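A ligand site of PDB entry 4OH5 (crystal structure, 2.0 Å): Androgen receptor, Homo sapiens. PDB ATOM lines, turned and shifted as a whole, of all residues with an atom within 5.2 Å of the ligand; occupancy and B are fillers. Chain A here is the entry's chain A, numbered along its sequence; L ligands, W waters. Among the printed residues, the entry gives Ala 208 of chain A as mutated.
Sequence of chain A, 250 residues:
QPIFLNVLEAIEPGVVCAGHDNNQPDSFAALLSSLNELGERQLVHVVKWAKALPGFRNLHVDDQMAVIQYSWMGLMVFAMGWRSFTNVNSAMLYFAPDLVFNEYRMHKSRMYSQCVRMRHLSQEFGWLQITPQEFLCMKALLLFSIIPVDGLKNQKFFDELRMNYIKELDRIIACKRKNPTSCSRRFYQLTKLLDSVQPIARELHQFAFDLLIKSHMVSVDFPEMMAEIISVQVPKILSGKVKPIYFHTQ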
ATOM      1  N   LEU A  32      26.023  10.313 -28.808  1.00  0.00           N
ATOM      2  CA  LEU A  32      24.838  10.897 -28.245  1.00  0.00           C
ATOM      3  C   LEU A  32      24.452  10.381 -26.880  1.00  0.00           C
ATOM      4  O   LEU A  32      24.022  11.159 -26.049  1.00  0.00           O
ATOM      5  CB  LEU A  32      23.702  10.770 -29.234  1.00  0.00           C
ATOM      6  CG  LEU A  32      23.878  11.929 -30.204  1.00  0.00           C
ATOM      7  CD1 LEU A  32      23.373  11.528 -31.549  1.00  0.00           C
ATOM      8  CD2 LEU A  32      23.133  13.148 -29.693  1.00  0.00           C
ATOM      9  N   LEU A  35      26.579  12.581 -24.896  1.00  0.00           N
ATOM     10  CA  LEU A  35      26.025  13.970 -24.774  1.00  0.00           C
ATOM     11  C   LEU A  35      24.877  14.008 -23.837  1.00  0.00           C
ATOM     12  O   LEU A  35      24.682  15.001 -23.176  1.00  0.00           O
ATOM     13  CB  LEU A  35      25.633  14.567 -26.137  1.00  0.00           C
ATOM     14  CG  LEU A  35      26.734  15.017 -27.100  1.00  0.00           C
ATOM     15  CD1 LEU A  35      26.276  15.181 -28.577  1.00  0.00           C
ATOM     16  CD2 LEU A  35      27.304  16.339 -26.599  1.00  0.00           C
ATOM     17  N   ASN A  36      24.075  12.916 -23.792  1.00  0.00           N
ATOM     18  CA  ASN A  36      22.872  12.850 -22.988  1.00  0.00           C
ATOM     19  C   ASN A  36      23.307  12.717 -21.536  1.00  0.00           C
ATOM     20  O   ASN A  36      22.867  13.485 -20.708  1.00  0.00           O
ATOM     21  CB  ASN A  36      22.016  11.660 -23.366  1.00  0.00           C
ATOM     22  CG  ASN A  36      21.221  11.887 -24.640  1.00  0.00           C
ATOM     23  OD1 ASN A  36      21.047  13.018 -25.128  1.00  0.00           O
ATOM     24  ND2 ASN A  36      20.622  10.821 -25.124  1.00  0.00           N
ATOM     25  N   LEU A  38      26.241  13.744 -20.347  1.00  0.00           N
ATOM     26  CA  LEU A  38      26.836  15.039 -20.047  1.00  0.00           C
ATOM     27  C   LEU A  38      25.766  16.068 -19.782  1.00  0.00           C
ATOM     28  O   LEU A  38      25.888  16.897 -18.882  1.00  0.00           O
ATOM     29  CB  LEU A  38      27.765  15.508 -21.173  1.00  0.00           C
ATOM     30  CG  LEU A  38      28.514  16.820 -20.912  1.00  0.00           C
ATOM     31  CD1 LEU A  38      29.410  16.777 -19.665  1.00  0.00           C
ATOM     32  CD2 LEU A  38      29.358  17.164 -22.114  1.00  0.00           C
ATOM     33  N   GLY A  39      24.676  16.017 -20.560  1.00  0.00           N
ATOM     34  CA  GLY A  39      23.531  16.923 -20.315  1.00  0.00           C
ATOM     35  C   GLY A  39      23.038  16.784 -18.865  1.00  0.00           C
ATOM     36  O   GLY A  39      22.785  17.774 -18.183  1.00  0.00           O
ATOM     37  N   GLN A  42      25.623  18.241 -16.348  1.00  0.00           N
ATOM     38  CA  GLN A  42      25.633  19.680 -16.364  1.00  0.00           C
ATOM     39  C   GLN A  42      24.355  20.274 -15.804  1.00  0.00           C
ATOM     40  O   GLN A  42      24.409  21.311 -15.176  1.00  0.00           O
ATOM     41  CB  GLN A  42      25.912  20.226 -17.750  1.00  0.00           C
ATOM     42  CG  GLN A  42      27.328  19.961 -18.210  1.00  0.00           C
ATOM     43  CD  GLN A  42      27.528  20.325 -19.642  1.00  0.00           C
ATOM     44  OE1 GLN A  42      28.617  20.133 -20.199  1.00  0.00           O
ATOM     45  NE2 GLN A  42      26.507  20.925 -20.245  1.00  0.00           N
ATOM     46  N   TRP A  72      17.894  25.743 -19.336  1.00  0.00           N
ATOM     47  CA  TRP A  72      19.007  24.826 -19.250  1.00  0.00           C
ATOM     48  C   TRP A  72      19.826  24.707 -20.594  1.00  0.00           C
ATOM     49  O   TRP A  72      21.024  24.783 -20.582  1.00  0.00           O
ATOM     50  CB  TRP A  72      18.412  23.451 -18.838  1.00  0.00           C
ATOM     51  CG  TRP A  72      19.131  22.292 -19.247  1.00  0.00           C
ATOM     52  CD1 TRP A  72      20.331  21.852 -18.757  1.00  0.00           C
ATOM     53  CD2 TRP A  72      18.732  21.367 -20.240  1.00  0.00           C
ATOM     54  NE1 TRP A  72      20.688  20.689 -19.375  1.00  0.00           N
ATOM     55  CE2 TRP A  72      19.737  20.376 -20.313  1.00  0.00           C
ATOM     56  CE3 TRP A  72      17.583  21.235 -21.059  1.00  0.00           C
ATOM     57  CZ2 TRP A  72      19.650  19.299 -21.209  1.00  0.00           C
ATOM     58  CZ3 TRP A  72      17.498  20.180 -21.935  1.00  0.00           C
ATOM     59  CH2 TRP A  72      18.522  19.209 -22.001  1.00  0.00           C
ATOM     60  N   MET A  73      19.159  24.381 -21.700  1.00  0.00           N
ATOM     61  CA  MET A  73      19.850  24.253 -23.015  1.00  0.00           C
ATOM     62  C   MET A  73      20.661  25.484 -23.436  1.00  0.00           C
ATOM     63  O   MET A  73      21.811  25.352 -23.804  1.00  0.00           O
ATOM     64  CB  MET A  73      18.857  23.820 -24.132  1.00  0.00           C
ATOM     65  CG  MET A  73      19.468  23.442 -25.465  1.00  0.00           C
ATOM     66  SD  MET A  73      20.592  22.070 -25.316  1.00  0.00           S
ATOM     67  CE  MET A  73      19.425  20.678 -25.200  1.00  0.00           C
ATOM     68  N   MET A  76      23.782  25.978 -21.263  1.00  0.00           N
ATOM     69  CA  MET A  76      24.798  24.983 -21.621  1.00  0.00           C
ATOM     70  C   MET A  76      25.491  25.415 -22.924  1.00  0.00           C
ATOM     71  O   MET A  76      26.725  25.308 -23.038  1.00  0.00           O
ATOM     72  CB  MET A  76      24.169  23.591 -21.809  1.00  0.00           C
ATOM     73  CG  MET A  76      23.708  22.800 -20.552  1.00  0.00           C
ATOM     74  SD  MET A  76      23.577  21.017 -20.820  1.00  0.00           S
ATOM     75  CE  MET A  76      22.528  20.829 -22.290  1.00  0.00           C
ATOM     76  N   VAL A  77      24.676  25.821 -23.925  1.00  0.00           N
ATOM     77  CA  VAL A  77      25.181  26.287 -25.210  1.00  0.00           C
ATOM     78  C   VAL A  77      26.134  27.423 -24.981  1.00  0.00           C
ATOM     79  O   VAL A  77      27.240  27.365 -25.471  1.00  0.00           O
ATOM     80  CB  VAL A  77      24.025  26.734 -26.172  1.00  0.00           C
ATOM     81  CG1 VAL A  77      24.603  27.509 -27.325  1.00  0.00           C
ATOM     82  CG2 VAL A  77      23.277  25.514 -26.648  1.00  0.00           C
ATOM     83  N   MET A  80      29.397  26.371 -23.177  1.00  0.00           N
ATOM     84  CA  MET A  80      30.184  25.517 -23.988  1.00  0.00           C
ATOM     85  C   MET A  80      30.911  26.364 -25.003  1.00  0.00           C
ATOM     86  O   MET A  80      32.097  26.132 -25.238  1.00  0.00           O
ATOM     87  CB  MET A  80      29.323  24.480 -24.654  1.00  0.00           C
ATOM     88  CG  MET A  80      30.046  23.369 -25.391  1.00  0.00           C
ATOM     89  SD  MET A  80      30.585  23.703 -27.100  1.00  0.00           S
ATOM     90  CE  MET A  80      29.032  23.686 -27.946  1.00  0.00           C
ATOM     91  N   ARG A  83      33.795  27.762 -23.276  1.00  0.00           N
ATOM     92  CA  ARG A  83      34.893  26.753 -23.055  1.00  0.00           C
ATOM     93  C   ARG A  83      35.629  26.460 -24.337  1.00  0.00           C
ATOM     94  O   ARG A  83      36.841  26.210 -24.353  1.00  0.00           O
ATOM     95  CB  ARG A  83      34.362  25.401 -22.595  1.00  0.00           C
ATOM     96  CG  ARG A  83      33.774  25.372 -21.232  1.00  0.00           C
ATOM     97  CD  ARG A  83      33.591  23.946 -20.707  1.00  0.00           C
ATOM     98  NE  ARG A  83      32.505  23.222 -21.389  1.00  0.00           N
ATOM     99  CZ  ARG A  83      31.208  23.416 -21.172  1.00  0.00           C
ATOM    100  NH1 ARG A  83      30.773  24.301 -20.318  1.00  0.00           N
ATOM    101  NH2 ARG A  83      30.332  22.652 -21.799  1.00  0.00           N
ATOM    102  N   TYR A  94      34.283  22.136 -27.389  1.00  0.00           N
ATOM    103  CA  TYR A  94      34.717  21.577 -26.107  1.00  0.00           C
ATOM    104  C   TYR A  94      33.511  21.306 -25.195  1.00  0.00           C
ATOM    105  O   TYR A  94      33.280  21.992 -24.185  1.00  0.00           O
ATOM    106  CB  TYR A  94      35.708  22.565 -25.487  1.00  0.00           C
ATOM    107  CG  TYR A  94      36.610  21.988 -24.408  1.00  0.00           C
ATOM    108  CD1 TYR A  94      37.936  21.652 -24.700  1.00  0.00           C
ATOM    109  CD2 TYR A  94      36.165  21.819 -23.124  1.00  0.00           C
ATOM    110  CE1 TYR A  94      38.797  21.170 -23.697  1.00  0.00           C
ATOM    111  CE2 TYR A  94      37.002  21.287 -22.144  1.00  0.00           C
ATOM    112  CZ  TYR A  94      38.314  20.970 -22.454  1.00  0.00           C
ATOM    113  OH  TYR A  94      39.119  20.495 -21.458  1.00  0.00           O
ATOM    114  N   PHE A  95      32.738  20.294 -25.558  1.00  0.00           N
ATOM    115  CA  PHE A  95      31.671  19.859 -24.705  1.00  0.00           C
ATOM    116  C   PHE A  95      32.177  19.513 -23.274  1.00  0.00           C
ATOM    117  O   PHE A  95      31.602  19.969 -22.275  1.00  0.00           O
ATOM    118  CB  PHE A  95      30.936  18.694 -25.321  1.00  0.00           C
ATOM    119  CG  PHE A  95      30.106  19.047 -26.511  1.00  0.00           C
ATOM    120  CD1 PHE A  95      30.592  18.836 -27.771  1.00  0.00           C
ATOM    121  CD2 PHE A  95      28.892  19.680 -26.367  1.00  0.00           C
ATOM    122  CE1 PHE A  95      29.793  19.106 -28.891  1.00  0.00           C
ATOM    123  CE2 PHE A  95      28.085  19.962 -27.471  1.00  0.00           C
ATOM    124  CZ  PHE A  95      28.557  19.696 -28.734  1.00  0.00           C
ATOM    125  N   MET A 111      24.535  16.250 -35.902  1.00  0.00           N
ATOM    126  CA  MET A 111      24.254  17.554 -35.321  1.00  0.00           C
ATOM    127  C   MET A 111      25.112  18.568 -35.976  1.00  0.00           C
ATOM    128  O   MET A 111      25.401  19.646 -35.420  1.00  0.00           O
ATOM    129  CB  MET A 111      24.552  17.601 -33.803  1.00  0.00           C
ATOM    130  CG  MET A 111      23.774  16.667 -32.953  1.00  0.00           C
ATOM    131  SD  MET A 111      24.278  16.604 -31.190  1.00  0.00           S
ATOM    132  CE  MET A 111      23.895  18.292 -30.767  1.00  0.00           C
ATOM    133  N   MET A 118      26.973  26.577 -33.164  1.00  0.00           N
ATOM    134  CA  MET A 118      27.650  26.792 -31.849  1.00  0.00           C
ATOM    135  C   MET A 118      29.104  27.203 -31.940  1.00  0.00           C
ATOM    136  O   MET A 118      29.597  28.017 -31.123  1.00  0.00           O
ATOM    137  CB  MET A 118      27.526  25.515 -31.006  1.00  0.00           C
ATOM    138  CG  MET A 118      26.094  25.212 -30.610  1.00  0.00           C
ATOM    139  SD  MET A 118      25.950  23.861 -29.434  1.00  0.00           S
ATOM    140  CE  MET A 118      26.015  22.413 -30.440  1.00  0.00           C
ATOM    141  N   LEU A 204      18.610  22.951 -30.839  1.00  0.00           N
ATOM    142  CA  LEU A 204      19.041  21.874 -29.958  1.00  0.00           C
ATOM    143  C   LEU A 204      17.840  21.212 -29.305  1.00  0.00           C
ATOM    144  O   LEU A 204      17.754  19.998 -29.204  1.00  0.00           O
ATOM    145  CB  LEU A 204      20.048  22.428 -28.967  1.00  0.00           C
ATOM    146  CG  LEU A 204      21.423  22.604 -29.660  1.00  0.00           C
ATOM    147  CD1 LEU A 204      22.272  23.573 -28.879  1.00  0.00           C
ATOM    148  CD2 LEU A 204      22.136  21.261 -29.805  1.00  0.00           C
ATOM    149  N   PHE A 207      16.151  18.882 -31.788  1.00  0.00           N
ATOM    150  CA  PHE A 207      16.993  17.693 -32.070  1.00  0.00           C
ATOM    151  C   PHE A 207      16.884  16.708 -30.939  1.00  0.00           C
ATOM    152  O   PHE A 207      16.714  15.453 -31.101  1.00  0.00           O
ATOM    153  CB  PHE A 207      18.470  18.132 -32.278  1.00  0.00           C
ATOM    154  CG  PHE A 207      19.427  16.985 -32.440  1.00  0.00           C
ATOM    155  CD1 PHE A 207      20.003  16.373 -31.345  1.00  0.00           C
ATOM    156  CD2 PHE A 207      19.711  16.482 -33.727  1.00  0.00           C
ATOM    157  CE1 PHE A 207      20.887  15.293 -31.498  1.00  0.00           C
ATOM    158  CE2 PHE A 207      20.574  15.383 -33.911  1.00  0.00           C
ATOM    159  CZ  PHE A 207      21.154  14.785 -32.783  1.00  0.00           C
ATOM    160  N   ALA A 208      17.009  17.250 -29.738  1.00  0.00           N
ATOM    161  CA  ALA A 208      16.903  16.452 -28.513  1.00  0.00           C
ATOM    162  C   ALA A 208      15.522  15.789 -28.421  1.00  0.00           C
ATOM    163  O   ALA A 208      15.395  14.581 -28.102  1.00  0.00           O
ATOM    164  CB  ALA A 208      17.138  17.334 -27.282  1.00  0.00           C
ATOM    165  N   LEU A 211      15.157  12.996 -31.026  1.00  0.00           N
ATOM    166  CA  LEU A 211      15.965  11.881 -30.622  1.00  0.00           C
ATOM    167  C   LEU A 211      15.319  11.131 -29.469  1.00  0.00           C
ATOM    168  O   LEU A 211      15.330   9.880 -29.415  1.00  0.00           O
ATOM    169  CB  LEU A 211      17.377  12.382 -30.236  1.00  0.00           C
ATOM    170  CG  LEU A 211      18.432  11.307 -29.966  1.00  0.00           C
ATOM    171  CD1 LEU A 211      18.588  10.381 -31.159  1.00  0.00           C
ATOM    172  CD2 LEU A 211      19.758  11.956 -29.654  1.00  0.00           C
ATOM    173  N   PHE A 222      18.770   7.659 -22.790  1.00  0.00           N
ATOM    174  CA  PHE A 222      18.454   8.889 -22.100  1.00  0.00           C
ATOM    175  C   PHE A 222      18.411   8.663 -20.627  1.00  0.00           C
ATOM    176  O   PHE A 222      17.675   7.806 -20.182  1.00  0.00           O
ATOM    177  CB  PHE A 222      17.124   9.475 -22.561  1.00  0.00           C
ATOM    178  CG  PHE A 222      17.230  10.223 -23.816  1.00  0.00           C
ATOM    179  CD1 PHE A 222      17.190   9.573 -25.028  1.00  0.00           C
ATOM    180  CD2 PHE A 222      17.378  11.612 -23.805  1.00  0.00           C
ATOM    181  CE1 PHE A 222      17.338  10.278 -26.218  1.00  0.00           C
ATOM    182  CE2 PHE A 222      17.507  12.304 -24.989  1.00  0.00           C
ATOM    183  CZ  PHE A 222      17.463  11.645 -26.197  1.00  0.00           C
ATOM    184  N   MET A 226      16.726  13.808 -18.136  1.00  0.00           N
ATOM    185  CA  MET A 226      16.783  14.240 -19.540  1.00  0.00           C
ATOM    186  C   MET A 226      15.482  13.822 -20.219  1.00  0.00           C
ATOM    187  O   MET A 226      14.859  14.612 -20.874  1.00  0.00           O
ATOM    188  CB  MET A 226      17.978  13.639 -20.293  1.00  0.00           C
ATOM    189  CG  MET A 226      19.342  14.231 -19.949  1.00  0.00           C
ATOM    190  SD  MET A 226      19.566  15.987 -20.373  1.00  0.00           S
ATOM    191  CE  MET A 226      19.321  16.697 -18.737  1.00  0.00           C
ATOM    192  N   ILE A 230      12.921  16.745 -21.434  1.00  0.00           N
ATOM    193  CA  ILE A 230      12.698  16.811 -22.839  1.00  0.00           C
ATOM    194  C   ILE A 230      11.235  16.436 -23.246  1.00  0.00           C
ATOM    195  O   ILE A 230      10.766  16.926 -24.223  1.00  0.00           O
ATOM    196  CB  ILE A 230      13.720  15.939 -23.580  1.00  0.00           C
ATOM    197  CG1 ILE A 230      15.171  16.397 -23.297  1.00  0.00           C
ATOM    198  CG2 ILE A 230      13.461  15.970 -25.080  1.00  0.00           C
ATOM    199  CD1 ILE A 230      16.223  15.468 -23.894  1.00  0.00           C
HETATM  200  F1  LIG L   1      24.597  21.805 -26.802  1.00  0.00           F
HETATM  201  C1  LIG L   1      25.234  22.003 -25.647  1.00  0.00           C
HETATM  202  F2  LIG L   1      24.686  22.981 -24.927  1.00  0.00           F
HETATM  203  F3  LIG L   1      26.476  22.421 -25.906  1.00  0.00           F
HETATM  204  C2  LIG L   1      25.206  20.670 -24.914  1.00  0.00           C
HETATM  205  C3  LIG L   1      24.281  19.641 -25.212  1.00  0.00           C
HETATM  206  C4  LIG L   1      26.214  20.411 -23.851  1.00  0.00           C
HETATM  207  N1  LIG L   1      27.192  21.348 -23.461  1.00  0.00           N
HETATM  208  O1  LIG L   1      28.444  20.929 -23.123  1.00  0.00           O
HETATM  209  O2  LIG L   1      27.011  22.512 -23.344  1.00  0.00           O
HETATM  210  C5  LIG L   1      26.173  19.175 -23.216  1.00  0.00           C
HETATM  211  C6  LIG L   1      25.241  18.182 -23.542  1.00  0.00           C
HETATM  212  C7  LIG L   1      24.262  18.387 -24.527  1.00  0.00           C
HETATM  213  N2  LIG L   1      23.351  17.351 -24.757  1.00  0.00           N
HETATM  214  C8  LIG L   1      22.303  17.501 -25.622  1.00  0.00           C
HETATM  215  O3  LIG L   1      22.043  18.573 -26.172  1.00  0.00           O
HETATM  216  C9  LIG L   1      21.346  16.383 -25.956  1.00  0.00           C
HETATM  217  C10 LIG L   1      20.122  16.255 -25.056  1.00  0.00           C
HETATM  218  C11 LIG L   1      21.500  15.520 -27.237  1.00  0.00           C
HETATM  219  O4  LIG L   1      22.067  15.294 -25.235  1.00  0.00           O
HETATM  220  O   HOH W   1      27.861  23.785 -20.845  1.00  0.00           O
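An oxygen (O1) of the ligand lies within hydrogen-bond range of the guanidinium group of Arg 83, at 2.9 Å. N2 of the ligand is in hydrogen-bond range of O of Leu 35 (3.1 Å). OD1 of Asn 36 lies within hydrogen-bond range of O4 of the ligand (2.5 Å). O4 of the ligand lies close to N of Asn 36 (3.4 Å). An oxygen (O1) of the ligand lies close to the side-chain amide oxygen (OE1) of Gln 42 (3.0 Å).
NH2 of Arg 83 lies within hydrogen-bond range of OE1 of Gln 42. The side-chain amide nitrogen of Gln 42 lies within hydrogen-bond range of the side-chain sulfur of Met 76. NE of Arg 83 lies within hydrogen-bond range of O of Tyr 94 (3.2 Å). The backbone carbonyl oxygen (O) of Phe 95 lies within hydrogen-bond range of the guanidinium group (NH2) of Arg 83 (3.0 Å). SD of Met 76 sits at hydrogen-bond distance from NE1 of Trp 72 (3.2 Å).
An oxygen (O2) of the ligand lies close to the backbone carbonyl oxygen (O) of Met 76 (2.8 Å). N of Val 77 lies close to F2 of the ligand. The backbone carbonyl oxygen of Phe 95 lies close to an oxygen (O1) of the ligand (3.4 Å). SD of Met 118 sits close to F1 of the ligand (3.6 Å). Merely in contact with the ligand: Leu 32 (3.8 Å), Leu 38 (3.9 Å), Gly 39 (3.7 Å), Met 73 (3.5 Å), Met 80 (3.3 Å), Leu 204 (3.6 Å) and Ala 208 (3.9 Å). 15 residues have an atom within 4 Å of the ligand: Leu 32, Leu 35, Asn 36, Leu 38, Gly 39, Gln 42, Met 73, Met 76, Val 77, Met 80, Arg 83, Phe 95, Met 118, Leu 204 and Ala 208. The nearest printed residue that does not touch the ligand is Ile 230 (4.1 Å).
Water W1 lies within hydrogen-bond range of the guanidinium group (NH2) of Arg 83 (2.9 Å), the backbone carbonyl oxygen (O) of Met 76 (2.9 Å), an oxygen (O2) of the ligand (2.9 Å) and the side-chain amide nitrogen (NE2) of Gln 42 (3.2 Å).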
